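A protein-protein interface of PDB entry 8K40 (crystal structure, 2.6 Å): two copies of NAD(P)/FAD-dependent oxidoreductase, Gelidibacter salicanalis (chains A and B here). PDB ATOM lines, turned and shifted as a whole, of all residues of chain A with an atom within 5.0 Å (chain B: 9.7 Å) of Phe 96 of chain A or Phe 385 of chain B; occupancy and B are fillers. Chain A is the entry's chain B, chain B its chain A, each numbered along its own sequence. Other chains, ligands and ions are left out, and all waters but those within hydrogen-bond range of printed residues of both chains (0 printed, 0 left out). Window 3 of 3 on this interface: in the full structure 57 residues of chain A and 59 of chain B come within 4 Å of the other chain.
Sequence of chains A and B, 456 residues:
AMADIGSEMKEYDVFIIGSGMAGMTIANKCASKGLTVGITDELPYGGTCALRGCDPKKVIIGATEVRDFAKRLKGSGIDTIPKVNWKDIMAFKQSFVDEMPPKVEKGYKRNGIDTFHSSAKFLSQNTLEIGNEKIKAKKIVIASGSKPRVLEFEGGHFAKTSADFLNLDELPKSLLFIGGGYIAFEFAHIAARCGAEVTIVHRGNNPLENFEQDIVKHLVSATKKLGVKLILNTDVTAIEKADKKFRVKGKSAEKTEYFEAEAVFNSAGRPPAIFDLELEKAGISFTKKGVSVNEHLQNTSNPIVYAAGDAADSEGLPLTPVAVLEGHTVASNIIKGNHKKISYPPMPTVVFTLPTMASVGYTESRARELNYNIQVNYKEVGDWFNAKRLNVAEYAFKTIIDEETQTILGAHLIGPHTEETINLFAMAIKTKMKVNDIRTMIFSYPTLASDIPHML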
ATOM      1  N   ASP A  55     -14.669   6.623 -20.904  1.00  0.00           N
ATOM      2  CA  ASP A  55     -13.779   5.693 -21.644  1.00  0.00           C
ATOM      3  C   ASP A  55     -14.114   5.722 -23.133  1.00  0.00           C
ATOM      4  O   ASP A  55     -13.270   6.143 -23.922  1.00  0.00           O
ATOM      5  CB  ASP A  55     -13.819   4.285 -21.061  1.00  0.00           C
ATOM      6  CG  ASP A  55     -12.924   4.119 -19.846  1.00  0.00           C
ATOM      7  OD1 ASP A  55     -12.595   5.162 -19.210  1.00  0.00           O
ATOM      8  OD2 ASP A  55     -12.552   2.944 -19.549  1.00  0.00           O
ATOM      9  N   LYS A  58     -13.412   9.063 -24.986  1.00  0.00           N
ATOM     10  CA  LYS A  58     -11.975   9.405 -25.133  1.00  0.00           C
ATOM     11  C   LYS A  58     -11.396   8.628 -26.313  1.00  0.00           C
ATOM     12  O   LYS A  58     -10.634   9.226 -27.108  1.00  0.00           O
ATOM     13  CB  LYS A  58     -11.183   9.097 -23.858  1.00  0.00           C
ATOM     14  CG  LYS A  58      -9.834   9.808 -23.736  1.00  0.00           C
ATOM     15  CD  LYS A  58      -9.890  11.336 -23.780  1.00  0.00           C
ATOM     16  CE  LYS A  58      -8.522  12.000 -23.730  1.00  0.00           C
ATOM     17  NZ  LYS A  58      -8.491  13.283 -24.485  1.00  0.00           N
ATOM     18  N   VAL A  59     -11.756   7.353 -26.455  1.00  0.00           N
ATOM     19  CA  VAL A  59     -11.346   6.551 -27.645  1.00  0.00           C
ATOM     20  C   VAL A  59     -11.714   7.314 -28.921  1.00  0.00           C
ATOM     21  O   VAL A  59     -10.825   7.500 -29.761  1.00  0.00           O
ATOM     22  CB  VAL A  59     -11.976   5.161 -27.665  1.00  0.00           C
ATOM     23  CG1 VAL A  59     -11.652   4.472 -28.979  1.00  0.00           C
ATOM     24  CG2 VAL A  59     -11.509   4.329 -26.487  1.00  0.00           C
ATOM     25  N   PHE A  92     -13.564   0.175 -33.143  1.00  0.00           N
ATOM     26  CA  PHE A  92     -12.409   0.327 -32.216  1.00  0.00           C
ATOM     27  C   PHE A  92     -12.947   0.649 -30.818  1.00  0.00           C
ATOM     28  O   PHE A  92     -12.579  -0.058 -29.856  1.00  0.00           O
ATOM     29  CB  PHE A  92     -11.420   1.390 -32.716  1.00  0.00           C
ATOM     30  CG  PHE A  92     -10.097   1.452 -31.987  1.00  0.00           C
ATOM     31  CD1 PHE A  92      -9.432   0.299 -31.599  1.00  0.00           C
ATOM     32  CD2 PHE A  92      -9.500   2.671 -31.710  1.00  0.00           C
ATOM     33  CE1 PHE A  92      -8.221   0.366 -30.928  1.00  0.00           C
ATOM     34  CE2 PHE A  92      -8.284   2.737 -31.045  1.00  0.00           C
ATOM     35  CZ  PHE A  92      -7.650   1.582 -30.647  1.00  0.00           C
ATOM     36  N   LYS A  93     -13.834   1.637 -30.717  1.00  0.00           N
ATOM     37  CA  LYS A  93     -14.548   1.967 -29.451  1.00  0.00           C
ATOM     38  C   LYS A  93     -15.259   0.715 -28.913  1.00  0.00           C
ATOM     39  O   LYS A  93     -15.148   0.449 -27.704  1.00  0.00           O
ATOM     40  CB  LYS A  93     -15.504   3.147 -29.666  1.00  0.00           C
ATOM     41  CG  LYS A  93     -16.216   3.652 -28.414  1.00  0.00           C
ATOM     42  CD  LYS A  93     -17.737   3.495 -28.436  1.00  0.00           C
ATOM     43  CE  LYS A  93     -18.184   2.062 -28.232  1.00  0.00           C
ATOM     44  NZ  LYS A  93     -19.564   1.818 -28.715  1.00  0.00           N
ATOM     45  N   GLN A  94     -15.960  -0.034 -29.767  1.00  0.00           N
ATOM     46  CA  GLN A  94     -16.832  -1.162 -29.339  1.00  0.00           C
ATOM     47  C   GLN A  94     -15.961  -2.269 -28.729  1.00  0.00           C
ATOM     48  O   GLN A  94     -16.390  -2.862 -27.729  1.00  0.00           O
ATOM     49  CB  GLN A  94     -17.699  -1.656 -30.511  1.00  0.00           C
ATOM     50  CG  GLN A  94     -18.987  -2.368 -30.105  1.00  0.00           C
ATOM     51  CD  GLN A  94     -19.929  -1.490 -29.307  1.00  0.00           C
ATOM     52  OE1 GLN A  94     -20.334  -0.402 -29.725  1.00  0.00           O
ATOM     53  NE2 GLN A  94     -20.269  -1.952 -28.120  1.00  0.00           N
ATOM     54  N   SER A  95     -14.788  -2.552 -29.297  1.00  0.00           N
ATOM     55  CA  SER A  95     -13.852  -3.591 -28.780  1.00  0.00           C
ATOM     56  C   SER A  95     -13.476  -3.280 -27.323  1.00  0.00           C
ATOM     57  O   SER A  95     -13.284  -4.219 -26.538  1.00  0.00           O
ATOM     58  CB  SER A  95     -12.619  -3.722 -29.651  1.00  0.00           C
ATOM     59  OG  SER A  95     -11.733  -2.621 -29.478  1.00  0.00           O
ATOM     60  N   PHE A  96     -13.365  -2.002 -26.970  1.00  0.00           N
ATOM     61  CA  PHE A  96     -13.048  -1.568 -25.588  1.00  0.00           C
ATOM     62  C   PHE A  96     -14.250  -1.878 -24.702  1.00  0.00           C
ATOM     63  O   PHE A  96     -14.073  -2.623 -23.729  1.00  0.00           O
ATOM     64  CB  PHE A  96     -12.662  -0.089 -25.524  1.00  0.00           C
ATOM     65  CG  PHE A  96     -11.246   0.160 -25.963  1.00  0.00           C
ATOM     66  CD1 PHE A  96     -10.186  -0.216 -25.155  1.00  0.00           C
ATOM     67  CD2 PHE A  96     -10.979   0.710 -27.206  1.00  0.00           C
ATOM     68  CE1 PHE A  96      -8.882  -0.015 -25.575  1.00  0.00           C
ATOM     69  CE2 PHE A  96      -9.672   0.902 -27.628  1.00  0.00           C
ATOM     70  CZ  PHE A  96      -8.628   0.543 -26.810  1.00  0.00           C
ATOM     71  N   VAL A  97     -15.420  -1.338 -25.058  1.00  0.00           N
ATOM     72  CA  VAL A  97     -16.706  -1.527 -24.317  1.00  0.00           C
ATOM     73  C   VAL A  97     -17.016  -3.032 -24.186  1.00  0.00           C
ATOM     74  O   VAL A  97     -17.276  -3.446 -23.062  1.00  0.00           O
ATOM     75  CB  VAL A  97     -17.856  -0.739 -24.973  1.00  0.00           C
ATOM     76  CG1 VAL A  97     -19.202  -1.047 -24.338  1.00  0.00           C
ATOM     77  CG2 VAL A  97     -17.596   0.761 -24.941  1.00  0.00           C
ATOM     78  N   ASP A  98     -16.936  -3.842 -25.249  1.00  0.00           N
ATOM     79  CA  ASP A  98     -17.391  -5.262 -25.198  1.00  0.00           C
ATOM     80  C   ASP A  98     -16.490  -6.131 -24.320  1.00  0.00           C
ATOM     81  O   ASP A  98     -16.976  -7.174 -23.855  1.00  0.00           O
ATOM     82  CB  ASP A  98     -17.465  -5.924 -26.577  1.00  0.00           C
ATOM     83  CG  ASP A  98     -18.555  -5.327 -27.444  1.00  0.00           C
ATOM     84  OD1 ASP A  98     -19.218  -4.391 -26.958  1.00  0.00           O
ATOM     85  OD2 ASP A  98     -18.725  -5.798 -28.588  1.00  0.00           O
ATOM     86  N   GLU A  99     -15.220  -5.773 -24.139  1.00  0.00           N
ATOM     87  CA  GLU A  99     -14.238  -6.682 -23.486  1.00  0.00           C
ATOM     88  C   GLU A  99     -14.262  -6.435 -21.976  1.00  0.00           C
ATOM     89  O   GLU A  99     -13.753  -7.303 -21.241  1.00  0.00           O
ATOM     90  CB  GLU A  99     -12.853  -6.537 -24.122  1.00  0.00           C
ATOM     91  CG  GLU A  99     -12.758  -7.249 -25.465  1.00  0.00           C
ATOM     92  CD  GLU A  99     -11.578  -6.889 -26.354  1.00  0.00           C
ATOM     93  OE1 GLU A  99     -10.569  -6.360 -25.836  1.00  0.00           O
ATOM     94  OE2 GLU A  99     -11.672  -7.143 -27.571  1.00  0.00           O
ATOM     95  N   MET A 100     -14.905  -5.348 -21.540  1.00  0.00           N
ATOM     96  CA  MET A 100     -14.881  -4.875 -20.127  1.00  0.00           C
ATOM     97  C   MET A 100     -15.822  -5.721 -19.255  1.00  0.00           C
ATOM     98  O   MET A 100     -15.366  -6.287 -18.261  1.00  0.00           O
ATOM     99  CB  MET A 100     -15.199  -3.370 -20.061  1.00  0.00           C
ATOM    100  CG  MET A 100     -15.324  -2.767 -18.661  1.00  0.00           C
ATOM    101  SD  MET A 100     -13.985  -3.130 -17.494  1.00  0.00           S
ATOM    102  CE  MET A 100     -12.525  -2.795 -18.481  1.00  0.00           C
ATOM    103  N   LEU B  73      -3.552   4.953 -35.534  1.00  0.00           N
ATOM    104  CA  LEU B  73      -5.023   4.739 -35.671  1.00  0.00           C
ATOM    105  C   LEU B  73      -5.385   4.343 -37.114  1.00  0.00           C
ATOM    106  O   LEU B  73      -6.583   4.426 -37.476  1.00  0.00           O
ATOM    107  CB  LEU B  73      -5.755   6.026 -35.268  1.00  0.00           C
ATOM    108  CG  LEU B  73      -5.552   6.489 -33.827  1.00  0.00           C
ATOM    109  CD1 LEU B  73      -6.522   7.604 -33.476  1.00  0.00           C
ATOM    110  CD2 LEU B  73      -5.702   5.334 -32.862  1.00  0.00           C
ATOM    111  N   SER B  76      -8.298   2.111 -37.823  1.00  0.00           N
ATOM    112  CA  SER B  76      -9.029   2.188 -36.533  1.00  0.00           C
ATOM    113  C   SER B  76      -9.739   3.550 -36.463  1.00  0.00           C
ATOM    114  O   SER B  76     -10.156   3.964 -35.355  1.00  0.00           O
ATOM    115  CB  SER B  76      -8.093   1.945 -35.355  1.00  0.00           C
ATOM    116  OG  SER B  76      -7.846   0.556 -35.140  1.00  0.00           O
ATOM    117  N   VAL B 381       3.296  -2.041 -19.153  1.00  0.00           N
ATOM    118  CA  VAL B 381       1.818  -1.870 -19.053  1.00  0.00           C
ATOM    119  C   VAL B 381       1.235  -1.373 -20.376  1.00  0.00           C
ATOM    120  O   VAL B 381       0.347  -0.524 -20.313  1.00  0.00           O
ATOM    121  CB  VAL B 381       1.486  -0.937 -17.880  1.00  0.00           C
ATOM    122  CG1 VAL B 381       1.857  -1.594 -16.566  1.00  0.00           C
ATOM    123  CG2 VAL B 381       2.151   0.415 -18.007  1.00  0.00           C
ATOM    124  N   GLY B 382       1.679  -1.960 -21.500  1.00  0.00           N
ATOM    125  CA  GLY B 382       1.151  -1.774 -22.870  1.00  0.00           C
ATOM    126  C   GLY B 382      -0.326  -2.129 -22.993  1.00  0.00           C
ATOM    127  O   GLY B 382      -0.991  -1.567 -23.899  1.00  0.00           O
ATOM    128  N   ASP B 383      -0.846  -2.993 -22.117  1.00  0.00           N
ATOM    129  CA  ASP B 383      -2.273  -3.422 -22.121  1.00  0.00           C
ATOM    130  C   ASP B 383      -3.163  -2.484 -21.275  1.00  0.00           C
ATOM    131  O   ASP B 383      -4.388  -2.671 -21.334  1.00  0.00           O
ATOM    132  CB  ASP B 383      -2.415  -4.905 -21.752  1.00  0.00           C
ATOM    133  CG  ASP B 383      -1.640  -5.351 -20.523  1.00  0.00           C
ATOM    134  OD1 ASP B 383      -0.500  -4.851 -20.329  1.00  0.00           O
ATOM    135  OD2 ASP B 383      -2.175  -6.208 -19.778  1.00  0.00           O
ATOM    136  N   TRP B 384      -2.613  -1.485 -20.565  1.00  0.00           N
ATOM    137  CA  TRP B 384      -3.390  -0.388 -19.905  1.00  0.00           C
ATOM    138  C   TRP B 384      -4.100   0.510 -20.928  1.00  0.00           C
ATOM    139  O   TRP B 384      -3.487   0.894 -21.967  1.00  0.00           O
ATOM    140  CB  TRP B 384      -2.506   0.485 -19.002  1.00  0.00           C
ATOM    141  CG  TRP B 384      -2.107  -0.146 -17.704  1.00  0.00           C
ATOM    142  CD1 TRP B 384      -2.247  -1.454 -17.336  1.00  0.00           C
ATOM    143  CD2 TRP B 384      -1.476   0.518 -16.598  1.00  0.00           C
ATOM    144  NE1 TRP B 384      -1.756  -1.644 -16.074  1.00  0.00           N
ATOM    145  CE2 TRP B 384      -1.267  -0.457 -15.600  1.00  0.00           C
ATOM    146  CE3 TRP B 384      -1.066   1.830 -16.358  1.00  0.00           C
ATOM    147  CZ2 TRP B 384      -0.661  -0.158 -14.381  1.00  0.00           C
ATOM    148  CZ3 TRP B 384      -0.467   2.129 -15.152  1.00  0.00           C
ATOM    149  CH2 TRP B 384      -0.268   1.147 -14.179  1.00  0.00           C
ATOM    150  N   PHE B 385      -5.313   0.939 -20.572  1.00  0.00           N
ATOM    151  CA  PHE B 385      -6.262   1.694 -21.432  1.00  0.00           C
ATOM    152  C   PHE B 385      -5.523   2.839 -22.133  1.00  0.00           C
ATOM    153  O   PHE B 385      -5.787   3.046 -23.338  1.00  0.00           O
ATOM    154  CB  PHE B 385      -7.470   2.173 -20.613  1.00  0.00           C
ATOM    155  CG  PHE B 385      -8.496   2.971 -21.383  1.00  0.00           C
ATOM    156  CD1 PHE B 385      -9.093   2.455 -22.522  1.00  0.00           C
ATOM    157  CD2 PHE B 385      -8.858   4.250 -20.981  1.00  0.00           C
ATOM    158  CE1 PHE B 385     -10.014   3.201 -23.243  1.00  0.00           C
ATOM    159  CE2 PHE B 385      -9.792   4.987 -21.693  1.00  0.00           C
ATOM    160  CZ  PHE B 385     -10.380   4.454 -22.813  1.00  0.00           C
ATOM    161  N   ASN B 386      -4.642   3.559 -21.428  1.00  0.00           N
ATOM    162  CA  ASN B 386      -4.095   4.838 -21.946  1.00  0.00           C
ATOM    163  C   ASN B 386      -3.213   4.526 -23.152  1.00  0.00           C
ATOM    164  O   ASN B 386      -3.271   5.292 -24.111  1.00  0.00           O
ATOM    165  CB  ASN B 386      -3.364   5.662 -20.884  1.00  0.00           C
ATOM    166  CG  ASN B 386      -4.305   6.557 -20.116  1.00  0.00           C
ATOM    167  OD1 ASN B 386      -5.292   7.038 -20.668  1.00  0.00           O
ATOM    168  ND2 ASN B 386      -4.004   6.785 -18.844  1.00  0.00           N
ATOM    169  N   ALA B 387      -2.433   3.452 -23.076  1.00  0.00           N
ATOM    170  CA  ALA B 387      -1.561   2.972 -24.172  1.00  0.00           C
ATOM    171  C   ALA B 387      -2.439   2.377 -25.277  1.00  0.00           C
ATOM    172  O   ALA B 387      -2.160   2.629 -26.452  1.00  0.00           O
ATOM    173  CB  ALA B 387      -0.551   1.964 -23.658  1.00  0.00           C
ATOM    174  N   LYS B 388      -3.476   1.627 -24.917  1.00  0.00           N
ATOM    175  CA  LYS B 388      -4.264   0.856 -25.913  1.00  0.00           C
ATOM    176  C   LYS B 388      -5.171   1.771 -26.737  1.00  0.00           C
ATOM    177  O   LYS B 388      -5.287   1.497 -27.940  1.00  0.00           O
ATOM    178  CB  LYS B 388      -4.990  -0.311 -25.243  1.00  0.00           C
ATOM    179  CG  LYS B 388      -4.102  -1.547 -25.176  1.00  0.00           C
ATOM    180  CD  LYS B 388      -4.784  -2.824 -24.796  1.00  0.00           C
ATOM    181  CE  LYS B 388      -4.456  -3.954 -25.750  1.00  0.00           C
ATOM    182  NZ  LYS B 388      -5.369  -5.103 -25.532  1.00  0.00           N
ATOM    183  N   ARG B 389      -5.755   2.821 -26.156  1.00  0.00           N
ATOM    184  CA  ARG B 389      -6.668   3.733 -26.895  1.00  0.00           C
ATOM    185  C   ARG B 389      -5.877   4.578 -27.890  1.00  0.00           C
ATOM    186  O   ARG B 389      -6.489   4.984 -28.892  1.00  0.00           O
ATOM    187  CB  ARG B 389      -7.448   4.663 -25.964  1.00  0.00           C
ATOM    188  CG  ARG B 389      -6.613   5.711 -25.246  1.00  0.00           C
ATOM    189  CD  ARG B 389      -7.453   6.383 -24.190  1.00  0.00           C
ATOM    190  NE  ARG B 389      -6.650   7.232 -23.339  1.00  0.00           N
ATOM    191  CZ  ARG B 389      -6.216   8.436 -23.664  1.00  0.00           C
ATOM    192  NH1 ARG B 389      -6.510   8.949 -24.844  1.00  0.00           N
ATOM    193  NH2 ARG B 389      -5.479   9.119 -22.804  1.00  0.00           N
ATOM    194  N   LEU B 390      -4.616   4.908 -27.575  1.00  0.00           N
ATOM    195  CA  LEU B 390      -3.711   5.714 -28.444  1.00  0.00           C
ATOM    196  C   LEU B 390      -2.899   4.743 -29.304  1.00  0.00           C
ATOM    197  O   LEU B 390      -2.174   5.218 -30.181  1.00  0.00           O
ATOM    198  CB  LEU B 390      -2.790   6.608 -27.605  1.00  0.00           C
ATOM    199  CG  LEU B 390      -3.459   7.732 -26.804  1.00  0.00           C
ATOM    200  CD1 LEU B 390      -2.416   8.625 -26.129  1.00  0.00           C
ATOM    201  CD2 LEU B 390      -4.380   8.589 -27.667  1.00  0.00           C
ATOM    202  N   ASN B 391      -3.065   3.438 -29.069  1.00  0.00           N
ATOM    203  CA  ASN B 391      -2.377   2.328 -29.784  1.00  0.00           C
ATOM    204  C   ASN B 391      -0.867   2.605 -29.795  1.00  0.00           C
ATOM    205  O   ASN B 391      -0.201   2.525 -30.862  1.00  0.00           O
ATOM    206  CB  ASN B 391      -2.979   2.069 -31.167  1.00  0.00           C
ATOM    207  CG  ASN B 391      -2.315   0.903 -31.869  1.00  0.00           C
ATOM    208  OD1 ASN B 391      -1.810  -0.013 -31.218  1.00  0.00           O
ATOM    209  ND2 ASN B 391      -2.263   0.961 -33.190  1.00  0.00           N
ATOM    210  N   VAL B 392      -0.350   2.915 -28.612  1.00  0.00           N
ATOM    211  CA  VAL B 392       1.105   3.017 -28.324  1.00  0.00           C
ATOM    212  C   VAL B 392       1.524   1.715 -27.655  1.00  0.00           C
ATOM    213  O   VAL B 392       1.077   1.472 -26.537  1.00  0.00           O
ATOM    214  CB  VAL B 392       1.405   4.240 -27.448  1.00  0.00           C
ATOM    215  CG1 VAL B 392       2.800   4.184 -26.856  1.00  0.00           C
ATOM    216  CG2 VAL B 392       1.190   5.523 -28.236  1.00  0.00           C
ATOM    217  N   TYR B 395       4.676   1.126 -23.207  1.00  0.00           N
ATOM    218  CA  TYR B 395       4.284   1.907 -22.022  1.00  0.00           C
ATOM    219  C   TYR B 395       4.798   1.127 -20.829  1.00  0.00           C
ATOM    220  O   TYR B 395       4.365  -0.026 -20.703  1.00  0.00           O
ATOM    221  CB  TYR B 395       2.776   2.129 -22.024  1.00  0.00           C
ATOM    222  CG  TYR B 395       2.224   2.985 -20.905  1.00  0.00           C
ATOM    223  CD1 TYR B 395       2.976   3.979 -20.286  1.00  0.00           C
ATOM    224  CD2 TYR B 395       0.898   2.861 -20.515  1.00  0.00           C
ATOM    225  CE1 TYR B 395       2.435   4.800 -19.305  1.00  0.00           C
ATOM    226  CE2 TYR B 395       0.349   3.650 -19.515  1.00  0.00           C
ATOM    227  CZ  TYR B 395       1.118   4.628 -18.910  1.00  0.00           C
ATOM    228  OH  TYR B 395       0.552   5.424 -17.952  1.00  0.00           O
ATOM    229  N   PRO B 416       3.008   7.412 -23.807  1.00  0.00           N
ATOM    230  CA  PRO B 416       2.392   8.694 -24.127  1.00  0.00           C
ATOM    231  C   PRO B 416       2.544   9.728 -23.001  1.00  0.00           C
ATOM    232  O   PRO B 416       2.433   9.372 -21.843  1.00  0.00           O
ATOM    233  CB  PRO B 416       0.917   8.373 -24.416  1.00  0.00           C
ATOM    234  CG  PRO B 416       0.696   6.939 -23.977  1.00  0.00           C
ATOM    235  CD  PRO B 416       2.052   6.295 -23.805  1.00  0.00           C
ATOM    236  N   TYR B 445      -9.612  12.453 -15.286  1.00  0.00           N
ATOM    237  CA  TYR B 445      -9.713  11.118 -15.943  1.00  0.00           C
ATOM    238  C   TYR B 445     -10.640  11.236 -17.147  1.00  0.00           C
ATOM    239  O   TYR B 445     -11.601  11.982 -17.074  1.00  0.00           O
ATOM    240  CB  TYR B 445     -10.263  10.079 -14.965  1.00  0.00           C
ATOM    241  CG  TYR B 445     -10.384   8.702 -15.543  1.00  0.00           C
ATOM    242  CD1 TYR B 445      -9.340   7.801 -15.457  1.00  0.00           C
ATOM    243  CD2 TYR B 445     -11.540   8.301 -16.192  1.00  0.00           C
ATOM    244  CE1 TYR B 445      -9.437   6.529 -16.008  1.00  0.00           C
ATOM    245  CE2 TYR B 445     -11.650   7.039 -16.760  1.00  0.00           C
ATOM    246  CZ  TYR B 445     -10.597   6.145 -16.667  1.00  0.00           C
ATOM    247  OH  TYR B 445     -10.721   4.902 -17.223  1.00  0.00           O
ATOM    248  N   PRO B 446     -10.411  10.555 -18.293  1.00  0.00           N
ATOM    249  CA  PRO B 446      -9.228   9.735 -18.541  1.00  0.00           C
ATOM    250  C   PRO B 446      -8.011  10.570 -18.981  1.00  0.00           C
ATOM    251  O   PRO B 446      -8.126  11.331 -19.931  1.00  0.00           O
ATOM    252  CB  PRO B 446      -9.655   8.797 -19.687  1.00  0.00           C
ATOM    253  CG  PRO B 446     -11.086   9.164 -20.037  1.00  0.00           C
ATOM    254  CD  PRO B 446     -11.326  10.533 -19.442  1.00  0.00           C
ATOM    255  N   THR B 447      -6.877  10.394 -18.302  1.00  0.00           N
ATOM    256  CA  THR B 447      -5.615  11.129 -18.557  1.00  0.00           C
ATOM    257  C   THR B 447      -4.438  10.245 -18.169  1.00  0.00           C
ATOM    258  O   THR B 447      -4.658   9.339 -17.374  1.00  0.00           O
ATOM    259  CB  THR B 447      -5.510  12.422 -17.744  1.00  0.00           C
ATOM    260  OG1 THR B 447      -5.292  12.017 -16.393  1.00  0.00           O
ATOM    261  CG2 THR B 447      -6.727  13.307 -17.876  1.00  0.00           C
ATOM    262  N   LEU B 448      -3.241  10.546 -18.677  1.00  0.00           N
ATOM    263  CA  LEU B 448      -2.004   9.780 -18.361  1.00  0.00           C
ATOM    264  C   LEU B 448      -1.602  10.038 -16.906  1.00  0.00           C
ATOM    265  O   LEU B 448      -1.081   9.116 -16.243  1.00  0.00           O
ATOM    266  CB  LEU B 448      -0.888  10.176 -19.328  1.00  0.00           C
ATOM    267  CG  LEU B 448      -0.851   9.396 -20.640  1.00  0.00           C
ATOM    268  CD1 LEU B 448      -0.475   7.940 -20.380  1.00  0.00           C
ATOM    269  CD2 LEU B 448      -2.185   9.501 -21.371  1.00  0.00           C
ATOM    270  N   SER B 450      -3.496  10.193 -14.447  1.00  0.00           N
ATOM    271  CA  SER B 450      -4.379   9.350 -13.600  1.00  0.00           C
ATOM    272  C   SER B 450      -3.810   7.937 -13.425  1.00  0.00           C
ATOM    273  O   SER B 450      -4.364   7.190 -12.584  1.00  0.00           O
ATOM    274  CB  SER B 450      -5.780   9.327 -14.144  1.00  0.00           C
ATOM    275  OG  SER B 450      -5.874   8.495 -15.289  1.00  0.00           O
ATOM    276  N   ASP B 451      -2.768   7.563 -14.174  1.00  0.00           N
ATOM    277  CA  ASP B 451      -2.067   6.260 -13.993  1.00  0.00           C
ATOM    278  C   ASP B 451      -1.010   6.364 -12.866  1.00  0.00           C
ATOM    279  O   ASP B 451      -0.566   5.302 -12.361  1.00  0.00           O
ATOM    280  CB  ASP B 451      -1.490   5.763 -15.320  1.00  0.00           C
ATOM    281  CG  ASP B 451      -2.526   5.321 -16.356  1.00  0.00           C
ATOM    282  OD1 ASP B 451      -3.656   4.943 -15.970  1.00  0.00           O
ATOM    283  OD2 ASP B 451      -2.182   5.335 -17.566  1.00  0.00           O
ATOM    284  N   HIS B 454      -1.247   4.116  -9.727  1.00  0.00           N
ATOM    285  CA  HIS B 454      -1.049   2.685 -10.062  1.00  0.00           C
ATOM    286  C   HIS B 454       0.445   2.397 -10.265  1.00  0.00           C
ATOM    287  O   HIS B 454       0.800   1.243 -10.545  1.00  0.00           O
ATOM    288  CB  HIS B 454      -1.931   2.332 -11.265  1.00  0.00           C
ATOM    289  CG  HIS B 454      -3.372   2.583 -10.978  1.00  0.00           C
ATOM    290  ND1 HIS B 454      -4.072   3.645 -11.551  1.00  0.00           N
ATOM    291  CD2 HIS B 454      -4.225   1.962 -10.129  1.00  0.00           C
ATOM    292  CE1 HIS B 454      -5.303   3.644 -11.099  1.00  0.00           C
ATOM    293  NE2 HIS B 454      -5.416   2.625 -10.211  1.00  0.00           N
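The side-chain carboxylate of Asp 55 of chain A is in hydrogen-bond range of the side-chain hydroxyl of Tyr 445 of chain B, 2.7 Å away.
OD1 of Asn 386 of chain B sits at hydrogen-bond distance from NH2 of Arg 389 of chain B, at 3.0 Å.
OG of Ser 95 of chain A lies within hydrogen-bond range of O of Phe 92 of chain A (2.7 Å).
CZ of Phe 385 of chain B touches O of Asp 55 of chain A (3.5 Å).
CG of Lys 58 of chain A touches NH1 of Arg 389 of chain B (3.6 Å).
Pro 446 of chain B touches Lys 58 of chain A (CG to CB, 3.8 Å).
Phe 385 of chain B touches Val 59 of chain A.
Phe 92 of chain A touches Ser 76 of chain B (CD1 to OG, 3.9 Å).
O of Lys 388 of chain B touches CZ of Phe 92 of chain A, 3.6 Å away.
Arg 389 of chain B touches Phe 92 of chain A (O to CE2, 3.6 Å).
Phe 385 of chain B touches Phe 96 of chain A (CD1 to CD1, 3.9 Å).
CZ of Phe 96 of chain A touches O of Lys 388 of chain B, 3.7 Å away.
Arg 389 of chain B touches Phe 96 of chain A.
Of the printed residues of chain B, Lys 58 of chain A touches Arg 389 (3.6 Å) and Pro 446 (3.8 Å).
Printed residues of chain B within 4 Å of Val 59 of chain A: Phe 385.
Phe 96 of chain A touches just these residues of chain B: Phe 385 (3.9 Å), Lys 388 (3.7 Å) and Arg 389 (3.7 Å).
No residue of chain B comes within 4 Å of Val 97 of chain A.
Of the printed residues of chain A, Ser 76 of chain B touches Phe 92 (3.9 Å).
Phe 385 of chain B touches just these residues of chain A: Asp 55, Val 59 and Phe 96.
The nearest residue of chain B that does not touch Phe 96 of chain A is Leu 390 of chain B (6.0 Å).
The nearest printed residue of chain B that does not touch Lys 58 of chain A is Phe 385 of chain B (4.8 Å).
Along chain A the printed residues that touch a printed residue of chain B span positions 55 to 96.
Among the printed residues, 11 pairs touch across the chains.
Among the printed residues, no Asp or Glu carboxylate lies within 4 Å of a Lys or Arg side-chain nitrogen of the other chain.
No position is printed for both chains.
Of the 11 pairs that touch across the chains among the printed residues, none has its exchanged pair printed and touching as well.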
